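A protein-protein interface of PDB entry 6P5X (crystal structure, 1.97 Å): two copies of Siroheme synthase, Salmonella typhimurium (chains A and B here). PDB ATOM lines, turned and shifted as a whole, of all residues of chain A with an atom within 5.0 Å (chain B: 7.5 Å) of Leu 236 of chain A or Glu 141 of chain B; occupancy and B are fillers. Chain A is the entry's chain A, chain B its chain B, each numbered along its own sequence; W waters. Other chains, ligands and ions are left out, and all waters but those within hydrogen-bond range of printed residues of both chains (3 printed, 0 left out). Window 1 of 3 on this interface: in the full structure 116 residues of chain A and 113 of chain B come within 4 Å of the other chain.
N of Leu 233 of chain B lies within hydrogen-bond range of O of Leu 231 of chain A, 2.9 Å away.
The backbone NH (N) of Leu 233 of chain A is in hydrogen-bond range of the backbone carbonyl oxygen (O) of Gly 229 of chain B (3.3 Å).
N of Lys 234 of chain A lies within hydrogen-bond range of O of Gly 229 of chain B.
The backbone carbonyl oxygen (O) of Gln 240 of chain A lies within hydrogen-bond range of the guanidinium group (NE) of Arg 137 of chain B (3.2 Å).
NH1 of Arg 140 of chain B sits close to NE2 of Gln 240 of chain A, 3.5 Å away.
The backbone NH (N) of Gly 235 of chain A lies within hydrogen-bond range of the side-chain hydroxyl (OG1) of Thr 232 of chain A, at 2.9 Å.
The side-chain amide nitrogen (NE2) of Gln 240 of chain A sits at hydrogen-bond distance from the backbone carbonyl oxygen (O) of Leu 258 of chain A (2.8 Å).
The side-chain carboxylate (OE2) of Glu 144 of chain B is in salt-bridge range of the guanidinium group (NH2) of Arg 140 of chain B (3.0 Å).
OG of Ser 145 of chain B is in hydrogen-bond range of O of Lys 142 of chain B.
Among the printed residues, merely in contact across the chains: Thr 232 of chain A with Gly 229 of chain B, Thr 232 of chain A with Leu 233 of chain B, Leu 233 of chain A with Ser 145 of chain B, Leu 233 of chain A with Leu 233 of chain B, Leu 236 of chain A with Glu 141 of chain B, Leu 236 of chain A with Ser 145 of chain B, Leu 236 of chain A with Leu 233 of chain B, Gln 237 of chain A with Glu 141 of chain B, Gln 240 of chain A with Glu 141 of chain B and Leu 258 of chain A with Glu 144 of chain B.
Printed residues of chain B within 4 Å of Leu 231 of chain A: Leu 233 (2.9 Å).
No residue of chain B comes within 4 Å of Gly 235 of chain A.
Leu 236 of chain A touches three residues of chain B.
Leu 135 of chain B touches none of the printed residues of chain A.
Leu 138 of chain B touches none of the printed residues of chain A.
Of chain A, only Leu 236 (3.6 Å), Gln 237 (3.3 Å) and Gln 240 (3.9 Å) come within 4 Å of Glu 141 of chain B.
Printed residues of chain A within 4 Å of Gly 229 of chain B: Thr 232 (3.5 Å), Leu 233 (3.3 Å) and Lys 234 (2.8 Å).
The nearest residue of chain B that does not touch Leu 236 of chain A is Glu 144 of chain B (4.6 Å).
The nearest residue of chain A that does not touch Glu 141 of chain B is Leu 233 of chain A (4.8 Å).
Of the 11 printed residues of chain A, 8 touch a printed residue of chain B.
Among the printed residues, no Asp or Glu carboxylate lies within 4 Å of a Lys or Arg side-chain nitrogen of the other chain.
Leu 233 of chain B touches its own counterpart, Leu 233 of chain A.
1 position is printed for both chains.
Water W1 lies within hydrogen-bond range of NE of Arg 137 of chain B (2.7 Å), OE1 of Glu 141 of chain B (3.0 Å) and OE1 of Gln 240 of chain A (3.1 Å).
Water W3 bridges O of Leu 233 of chain A (2.9 Å) and OE2 of Glu 141 of chain B (2.9 Å).
Water W2 lies within hydrogen-bond range of OE1 of Gln 240 of chain A (2.9 Å) and NH1 of Arg 140 of chain B (3.0 Å).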
ATOM      1  N   LEU A 231     -11.411 -18.369   7.838  1.00  0.00           N
ATOM      2  CA  LEU A 231     -12.676 -19.029   7.531  1.00  0.00           C
ATOM      3  C   LEU A 231     -13.108 -18.637   6.117  1.00  0.00           C
ATOM      4  O   LEU A 231     -12.836 -17.521   5.655  1.00  0.00           O
ATOM      5  CB  LEU A 231     -13.734 -18.639   8.570  1.00  0.00           C
ATOM      6  CG  LEU A 231     -15.132 -19.244   8.451  1.00  0.00           C
ATOM      7  CD1 LEU A 231     -15.136 -20.762   8.730  1.00  0.00           C
ATOM      8  CD2 LEU A 231     -16.089 -18.509   9.407  1.00  0.00           C
ATOM      9  N   THR A 232     -13.757 -19.569   5.404  1.00  0.00           N
ATOM     10  CA  THR A 232     -14.257 -19.258   4.064  1.00  0.00           C
ATOM     11  C   THR A 232     -15.563 -18.477   4.161  1.00  0.00           C
ATOM     12  O   THR A 232     -16.287 -18.577   5.141  1.00  0.00           O
ATOM     13  CB  THR A 232     -14.533 -20.522   3.249  1.00  0.00           C
ATOM     14  OG1 THR A 232     -15.459 -21.346   3.973  1.00  0.00           O
ATOM     15  CG2 THR A 232     -13.243 -21.313   2.980  1.00  0.00           C
ATOM     16  N   LEU A 233     -15.884 -17.725   3.102  1.00  0.00           N
ATOM     17  CA  LEU A 233     -17.181 -17.052   3.044  1.00  0.00           C
ATOM     18  C   LEU A 233     -18.322 -18.039   3.234  1.00  0.00           C
ATOM     19  O   LEU A 233     -19.291 -17.751   3.942  1.00  0.00           O
ATOM     20  CB  LEU A 233     -17.320 -16.313   1.709  1.00  0.00           C
ATOM     21  CG  LEU A 233     -16.326 -15.160   1.588  1.00  0.00           C
ATOM     22  CD1 LEU A 233     -16.258 -14.660   0.157  1.00  0.00           C
ATOM     23  CD2 LEU A 233     -16.696 -14.026   2.566  1.00  0.00           C
ATOM     24  N   LYS A 234     -18.232 -19.209   2.597  1.00  0.00           N
ATOM     25  CA  LYS A 234     -19.314 -20.182   2.710  1.00  0.00           C
ATOM     26  C   LYS A 234     -19.358 -20.791   4.102  1.00  0.00           C
ATOM     27  O   LYS A 234     -20.444 -21.040   4.630  1.00  0.00           O
ATOM     28  CB  LYS A 234     -19.175 -21.270   1.641  1.00  0.00           C
ATOM     29  CG  LYS A 234     -20.349 -22.253   1.640  1.00  0.00           C
ATOM     30  CD  LYS A 234     -20.398 -23.085   0.373  1.00  0.00           C
ATOM     31  CE  LYS A 234     -21.560 -24.079   0.440  1.00  0.00           C
ATOM     32  NZ  LYS A 234     -21.489 -25.120  -0.624  1.00  0.00           N
ATOM     33  N   GLY A 235     -18.196 -21.004   4.729  1.00  0.00           N
ATOM     34  CA  GLY A 235     -18.193 -21.483   6.096  1.00  0.00           C
ATOM     35  C   GLY A 235     -18.860 -20.507   7.049  1.00  0.00           C
ATOM     36  O   GLY A 235     -19.615 -20.908   7.937  1.00  0.00           O
ATOM     37  N   LEU A 236     -18.598 -19.209   6.866  1.00  0.00           N
ATOM     38  CA  LEU A 236     -19.271 -18.195   7.674  1.00  0.00           C
ATOM     39  C   LEU A 236     -20.773 -18.250   7.451  1.00  0.00           C
ATOM     40  O   LEU A 236     -21.557 -18.235   8.407  1.00  0.00           O
ATOM     41  CB  LEU A 236     -18.711 -16.811   7.330  1.00  0.00           C
ATOM     42  CG  LEU A 236     -19.357 -15.619   8.059  1.00  0.00           C
ATOM     43  CD1 LEU A 236     -19.126 -15.703   9.561  1.00  0.00           C
ATOM     44  CD2 LEU A 236     -18.818 -14.301   7.484  1.00  0.00           C
ATOM     45  N   GLN A 237     -21.189 -18.346   6.189  1.00  0.00           N
ATOM     46  CA  GLN A 237     -22.609 -18.473   5.871  1.00  0.00           C
ATOM     47  C   GLN A 237     -23.243 -19.652   6.605  1.00  0.00           C
ATOM     48  O   GLN A 237     -24.307 -19.514   7.219  1.00  0.00           O
ATOM     49  CB  GLN A 237     -22.787 -18.630   4.360  1.00  0.00           C
ATOM     50  CG  GLN A 237     -24.234 -18.730   3.886  1.00  0.00           C
ATOM     51  CD  GLN A 237     -24.332 -18.999   2.393  1.00  0.00           C
ATOM     52  OE1 GLN A 237     -24.665 -18.109   1.615  1.00  0.00           O
ATOM     53  NE2 GLN A 237     -24.034 -20.231   1.988  1.00  0.00           N
ATOM     54  N   GLN A 238     -22.597 -20.825   6.564  1.00  0.00           N
ATOM     55  CA  GLN A 238     -23.218 -22.007   7.162  1.00  0.00           C
ATOM     56  C   GLN A 238     -23.317 -21.888   8.679  1.00  0.00           C
ATOM     57  O   GLN A 238     -24.337 -22.279   9.275  1.00  0.00           O
ATOM     58  CB  GLN A 238     -22.447 -23.269   6.771  1.00  0.00           C
ATOM     59  CG  GLN A 238     -22.355 -23.519   5.257  1.00  0.00           C
ATOM     60  CD  GLN A 238     -23.617 -24.122   4.661  1.00  0.00           C
ATOM     61  OE1 GLN A 238     -24.673 -24.088   5.271  1.00  0.00           O
ATOM     62  NE2 GLN A 238     -23.501 -24.688   3.463  1.00  0.00           N
ATOM     63  N   ILE A 239     -22.278 -21.368   9.339  1.00  0.00           N
ATOM     64  CA  ILE A 239     -22.375 -21.277  10.794  1.00  0.00           C
ATOM     65  C   ILE A 239     -23.330 -20.170  11.200  1.00  0.00           C
ATOM     66  O   ILE A 239     -23.891 -20.212  12.300  1.00  0.00           O
ATOM     67  CB  ILE A 239     -21.012 -21.063  11.484  1.00  0.00           C
ATOM     68  CG1 ILE A 239     -20.358 -19.746  11.053  1.00  0.00           C
ATOM     69  CG2 ILE A 239     -20.082 -22.259  11.222  1.00  0.00           C
ATOM     70  CD1 ILE A 239     -18.996 -19.508  11.706  1.00  0.00           C
ATOM     71  N   GLN A 240     -23.533 -19.178  10.341  1.00  0.00           N
ATOM     72  CA  GLN A 240     -24.475 -18.106  10.661  1.00  0.00           C
ATOM     73  C   GLN A 240     -25.930 -18.521  10.525  1.00  0.00           C
ATOM     74  O   GLN A 240     -26.811 -17.784  10.985  1.00  0.00           O
ATOM     75  CB  GLN A 240     -24.204 -16.901   9.763  1.00  0.00           C
ATOM     76  CG  GLN A 240     -23.122 -16.006  10.298  1.00  0.00           C
ATOM     77  CD  GLN A 240     -23.647 -15.139  11.401  1.00  0.00           C
ATOM     78  OE1 GLN A 240     -24.744 -14.599  11.291  1.00  0.00           O
ATOM     79  NE2 GLN A 240     -22.879 -15.004  12.484  1.00  0.00           N
ATOM     80  N   LEU A 258     -18.128 -16.189  15.605  1.00  0.00           N
ATOM     81  CA  LEU A 258     -18.800 -15.958  14.327  1.00  0.00           C
ATOM     82  C   LEU A 258     -20.025 -16.842  14.131  1.00  0.00           C
ATOM     83  O   LEU A 258     -20.720 -16.713  13.114  1.00  0.00           O
ATOM     84  CB  LEU A 258     -17.813 -16.176  13.174  1.00  0.00           C
ATOM     85  CG  LEU A 258     -16.709 -15.110  13.078  1.00  0.00           C
ATOM     86  CD1 LEU A 258     -15.743 -15.447  11.972  1.00  0.00           C
ATOM     87  CD2 LEU A 258     -17.326 -13.727  12.844  1.00  0.00           C
ATOM     88  N   SER B 115     -28.268  -6.597  16.327  1.00  0.00           N
ATOM     89  CA  SER B 115     -27.135  -7.457  16.008  1.00  0.00           C
ATOM     90  C   SER B 115     -25.863  -6.618  16.031  1.00  0.00           C
ATOM     91  O   SER B 115     -25.859  -5.473  15.576  1.00  0.00           O
ATOM     92  CB  SER B 115     -27.309  -8.123  14.638  1.00  0.00           C
ATOM     93  OG  SER B 115     -27.091  -7.194  13.590  1.00  0.00           O
ATOM     94  N   ILE B 117     -21.574  -6.117  15.654  1.00  0.00           N
ATOM     95  CA  ILE B 117     -20.276  -6.469  15.076  1.00  0.00           C
ATOM     96  C   ILE B 117     -19.243  -5.744  15.929  1.00  0.00           C
ATOM     97  O   ILE B 117     -19.216  -4.502  15.951  1.00  0.00           O
ATOM     98  CB  ILE B 117     -20.163  -6.073  13.594  1.00  0.00           C
ATOM     99  CG1 ILE B 117     -21.299  -6.681  12.761  1.00  0.00           C
ATOM    100  CG2 ILE B 117     -18.799  -6.483  13.041  1.00  0.00           C
ATOM    101  CD1 ILE B 117     -22.570  -5.807  12.669  1.00  0.00           C
ATOM    102  N   LEU B 135     -33.055 -10.100   8.832  1.00  0.00           N
ATOM    103  CA  LEU B 135     -32.297  -9.126   8.051  1.00  0.00           C
ATOM    104  C   LEU B 135     -31.132  -8.582   8.864  1.00  0.00           C
ATOM    105  O   LEU B 135     -30.018  -8.450   8.341  1.00  0.00           O
ATOM    106  CB  LEU B 135     -33.201  -7.995   7.583  1.00  0.00           C
ATOM    107  CG  LEU B 135     -32.519  -6.916   6.752  1.00  0.00           C
ATOM    108  CD1 LEU B 135     -31.882  -7.527   5.500  1.00  0.00           C
ATOM    109  CD2 LEU B 135     -33.564  -5.873   6.386  1.00  0.00           C
ATOM    110  N   ALA B 136     -31.354  -8.328  10.160  1.00  0.00           N
ATOM    111  CA  ALA B 136     -30.267  -7.887  11.035  1.00  0.00           C
ATOM    112  C   ALA B 136     -29.153  -8.930  11.095  1.00  0.00           C
ATOM    113  O   ALA B 136     -27.967  -8.586  11.045  1.00  0.00           O
ATOM    114  CB  ALA B 136     -30.803  -7.573  12.437  1.00  0.00           C
ATOM    115  N   ARG B 137     -29.515 -10.214  11.179  1.00  0.00           N
ATOM    116  CA  ARG B 137     -28.515 -11.277  11.195  1.00  0.00           C
ATOM    117  C   ARG B 137     -27.753 -11.358   9.876  1.00  0.00           C
ATOM    118  O   ARG B 137     -26.526 -11.539   9.864  1.00  0.00           O
ATOM    119  CB  ARG B 137     -29.192 -12.612  11.495  1.00  0.00           C
ATOM    120  CG  ARG B 137     -28.255 -13.655  12.053  1.00  0.00           C
ATOM    121  CD  ARG B 137     -28.815 -15.033  11.765  1.00  0.00           C
ATOM    122  NE  ARG B 137     -28.774 -15.332  10.335  1.00  0.00           N
ATOM    123  CZ  ARG B 137     -29.652 -16.104   9.700  1.00  0.00           C
ATOM    124  NH1 ARG B 137     -30.666 -16.642  10.369  1.00  0.00           N
ATOM    125  NH2 ARG B 137     -29.516 -16.333   8.396  1.00  0.00           N
ATOM    126  N   LEU B 138     -28.475 -11.312   8.747  1.00  0.00           N
ATOM    127  CA  LEU B 138     -27.811 -11.369   7.446  1.00  0.00           C
ATOM    128  C   LEU B 138     -26.846 -10.199   7.263  1.00  0.00           C
ATOM    129  O   LEU B 138     -25.763 -10.351   6.681  1.00  0.00           O
ATOM    130  CB  LEU B 138     -28.851 -11.372   6.329  1.00  0.00           C
ATOM    131  CG  LEU B 138     -29.765 -12.604   6.228  1.00  0.00           C
ATOM    132  CD1 LEU B 138     -30.908 -12.356   5.270  1.00  0.00           C
ATOM    133  CD2 LEU B 138     -28.969 -13.830   5.779  1.00  0.00           C
ATOM    134  N   LEU B 139     -27.225  -9.021   7.736  1.00  0.00           N
ATOM    135  CA  LEU B 139     -26.314  -7.883   7.634  1.00  0.00           C
ATOM    136  C   LEU B 139     -25.131  -8.030   8.574  1.00  0.00           C
ATOM    137  O   LEU B 139     -24.021  -7.609   8.241  1.00  0.00           O
ATOM    138  CB  LEU B 139     -27.056  -6.577   7.916  1.00  0.00           C
ATOM    139  CG  LEU B 139     -28.049  -6.232   6.797  1.00  0.00           C
ATOM    140  CD1 LEU B 139     -28.877  -5.012   7.166  1.00  0.00           C
ATOM    141  CD2 LEU B 139     -27.339  -6.004   5.463  1.00  0.00           C
ATOM    142  N   ARG B 140     -25.334  -8.636   9.742  1.00  0.00           N
ATOM    143  CA  ARG B 140     -24.189  -8.927  10.604  1.00  0.00           C
ATOM    144  C   ARG B 140     -23.200  -9.856   9.905  1.00  0.00           C
ATOM    145  O   ARG B 140     -21.988  -9.609   9.938  1.00  0.00           O
ATOM    146  CB  ARG B 140     -24.637  -9.543  11.926  1.00  0.00           C
ATOM    147  CG  ARG B 140     -23.442  -9.742  12.850  1.00  0.00           C
ATOM    148  CD  ARG B 140     -23.658 -10.750  13.970  1.00  0.00           C
ATOM    149  NE  ARG B 140     -22.353 -11.093  14.532  1.00  0.00           N
ATOM    150  CZ  ARG B 140     -22.081 -12.210  15.194  1.00  0.00           C
ATOM    151  NH1 ARG B 140     -23.020 -13.121  15.404  1.00  0.00           N
ATOM    152  NH2 ARG B 140     -20.851 -12.417  15.632  1.00  0.00           N
ATOM    153  N   GLU B 141     -23.704 -10.915   9.260  1.00  0.00           N
ATOM    154  CA  GLU B 141     -22.840 -11.827   8.511  1.00  0.00           C
ATOM    155  C   GLU B 141     -22.031 -11.080   7.457  1.00  0.00           C
ATOM    156  O   GLU B 141     -20.812 -11.271   7.340  1.00  0.00           O
ATOM    157  CB  GLU B 141     -23.674 -12.926   7.852  1.00  0.00           C
ATOM    158  CG  GLU B 141     -22.873 -13.756   6.876  1.00  0.00           C
ATOM    159  CD  GLU B 141     -23.740 -14.741   6.104  1.00  0.00           C
ATOM    160  OE1 GLU B 141     -24.932 -14.899   6.455  1.00  0.00           O
ATOM    161  OE2 GLU B 141     -23.223 -15.355   5.146  1.00  0.00           O
ATOM    162  N   LYS B 142     -22.697 -10.224   6.674  1.00  0.00           N
ATOM    163  CA  LYS B 142     -22.003  -9.436   5.654  1.00  0.00           C
ATOM    164  C   LYS B 142     -20.934  -8.544   6.277  1.00  0.00           C
ATOM    165  O   LYS B 142     -19.780  -8.508   5.820  1.00  0.00           O
ATOM    166  CB  LYS B 142     -23.016  -8.597   4.878  1.00  0.00           C
ATOM    167  CG  LYS B 142     -22.380  -7.623   3.892  1.00  0.00           C
ATOM    168  CD  LYS B 142     -21.550  -8.340   2.853  1.00  0.00           C
ATOM    169  CE  LYS B 142     -22.370  -8.650   1.615  1.00  0.00           C
ATOM    170  NZ  LYS B 142     -21.558  -9.335   0.574  1.00  0.00           N
ATOM    171  N   LEU B 143     -21.293  -7.818   7.335  1.00  0.00           N
ATOM    172  CA  LEU B 143     -20.332  -6.908   7.960  1.00  0.00           C
ATOM    173  C   LEU B 143     -19.186  -7.659   8.634  1.00  0.00           C
ATOM    174  O   LEU B 143     -18.038  -7.184   8.626  1.00  0.00           O
ATOM    175  CB  LEU B 143     -21.056  -6.011   8.962  1.00  0.00           C
ATOM    176  CG  LEU B 143     -22.098  -5.135   8.267  1.00  0.00           C
ATOM    177  CD1 LEU B 143     -22.742  -4.163   9.231  1.00  0.00           C
ATOM    178  CD2 LEU B 143     -21.471  -4.403   7.110  1.00  0.00           C
ATOM    179  N   GLU B 144     -19.471  -8.815   9.245  1.00  0.00           N
ATOM    180  CA  GLU B 144     -18.390  -9.594   9.841  1.00  0.00           C
ATOM    181  C   GLU B 144     -17.381 -10.029   8.792  1.00  0.00           C
ATOM    182  O   GLU B 144     -16.185 -10.096   9.086  1.00  0.00           O
ATOM    183  CB  GLU B 144     -18.916 -10.839  10.560  1.00  0.00           C
ATOM    184  CG  GLU B 144     -19.734 -10.563  11.821  1.00  0.00           C
ATOM    185  CD  GLU B 144     -18.898 -10.286  13.072  1.00  0.00           C
ATOM    186  OE1 GLU B 144     -17.644 -10.153  12.980  1.00  0.00           O
ATOM    187  OE2 GLU B 144     -19.517 -10.208  14.159  1.00  0.00           O
ATOM    188  N   SER B 145     -17.838 -10.348   7.576  1.00  0.00           N
ATOM    189  CA  SER B 145     -16.891 -10.788   6.556  1.00  0.00           C
ATOM    190  C   SER B 145     -16.060  -9.624   6.035  1.00  0.00           C
ATOM    191  O   SER B 145     -14.941  -9.831   5.551  1.00  0.00           O
ATOM    192  CB  SER B 145     -17.616 -11.452   5.393  1.00  0.00           C
ATOM    193  OG  SER B 145     -18.333 -10.509   4.612  1.00  0.00           O
ATOM    194  N   LEU B 146     -16.584  -8.402   6.129  1.00  0.00           N
ATOM    195  CA  LEU B 146     -15.937  -7.239   5.521  1.00  0.00           C
ATOM    196  C   LEU B 146     -15.006  -6.482   6.461  1.00  0.00           C
ATOM    197  O   LEU B 146     -14.067  -5.828   5.990  1.00  0.00           O
ATOM    198  CB  LEU B 146     -16.999  -6.286   4.991  1.00  0.00           C
ATOM    199  CG  LEU B 146     -17.676  -6.853   3.737  1.00  0.00           C
ATOM    200  CD1 LEU B 146     -18.797  -5.960   3.282  1.00  0.00           C
ATOM    201  CD2 LEU B 146     -16.649  -7.065   2.605  1.00  0.00           C
ATOM    202  N   LEU B 147     -15.244  -6.526   7.769  1.00  0.00           N
ATOM    203  CA  LEU B 147     -14.431  -5.767   8.711  1.00  0.00           C
ATOM    204  C   LEU B 147     -13.281  -6.630   9.206  1.00  0.00           C
ATOM    205  O   LEU B 147     -13.532  -7.665   9.841  1.00  0.00           O
ATOM    206  CB  LEU B 147     -15.279  -5.298   9.891  1.00  0.00           C
ATOM    207  CG  LEU B 147     -16.370  -4.286   9.511  1.00  0.00           C
ATOM    208  CD1 LEU B 147     -17.152  -3.879  10.754  1.00  0.00           C
ATOM    209  CD2 LEU B 147     -15.742  -3.057   8.865  1.00  0.00           C
ATOM    210  N   GLY B 229     -17.471 -18.918  -2.932  1.00  0.00           N
ATOM    211  CA  GLY B 229     -17.662 -19.047  -1.492  1.00  0.00           C
ATOM    212  C   GLY B 229     -16.461 -19.612  -0.751  1.00  0.00           C
ATOM    213  O   GLY B 229     -16.458 -19.609   0.485  1.00  0.00           O
ATOM    214  N   LEU B 233     -12.281 -14.952   4.372  1.00  0.00           N
ATOM    215  CA  LEU B 233     -12.672 -13.588   4.752  1.00  0.00           C
ATOM    216  C   LEU B 233     -11.527 -12.604   4.521  1.00  0.00           C
ATOM    217  O   LEU B 233     -11.722 -11.524   3.938  1.00  0.00           O
ATOM    218  CB  LEU B 233     -13.135 -13.548   6.223  1.00  0.00           C
ATOM    219  CG  LEU B 233     -14.126 -14.612   6.743  1.00  0.00           C
ATOM    220  CD1 LEU B 233     -14.629 -14.235   8.144  1.00  0.00           C
ATOM    221  CD2 LEU B 233     -15.296 -14.891   5.832  1.00  0.00           C
HETATM  222  O   HOH W   1     -26.683 -14.638   8.829  1.00  0.00           O
HETATM  223  O   HOH W   2     -25.489 -14.168  14.030  1.00  0.00           O
HETATM  224  O   HOH W   3     -20.532 -15.171   4.024  1.00  0.00           O
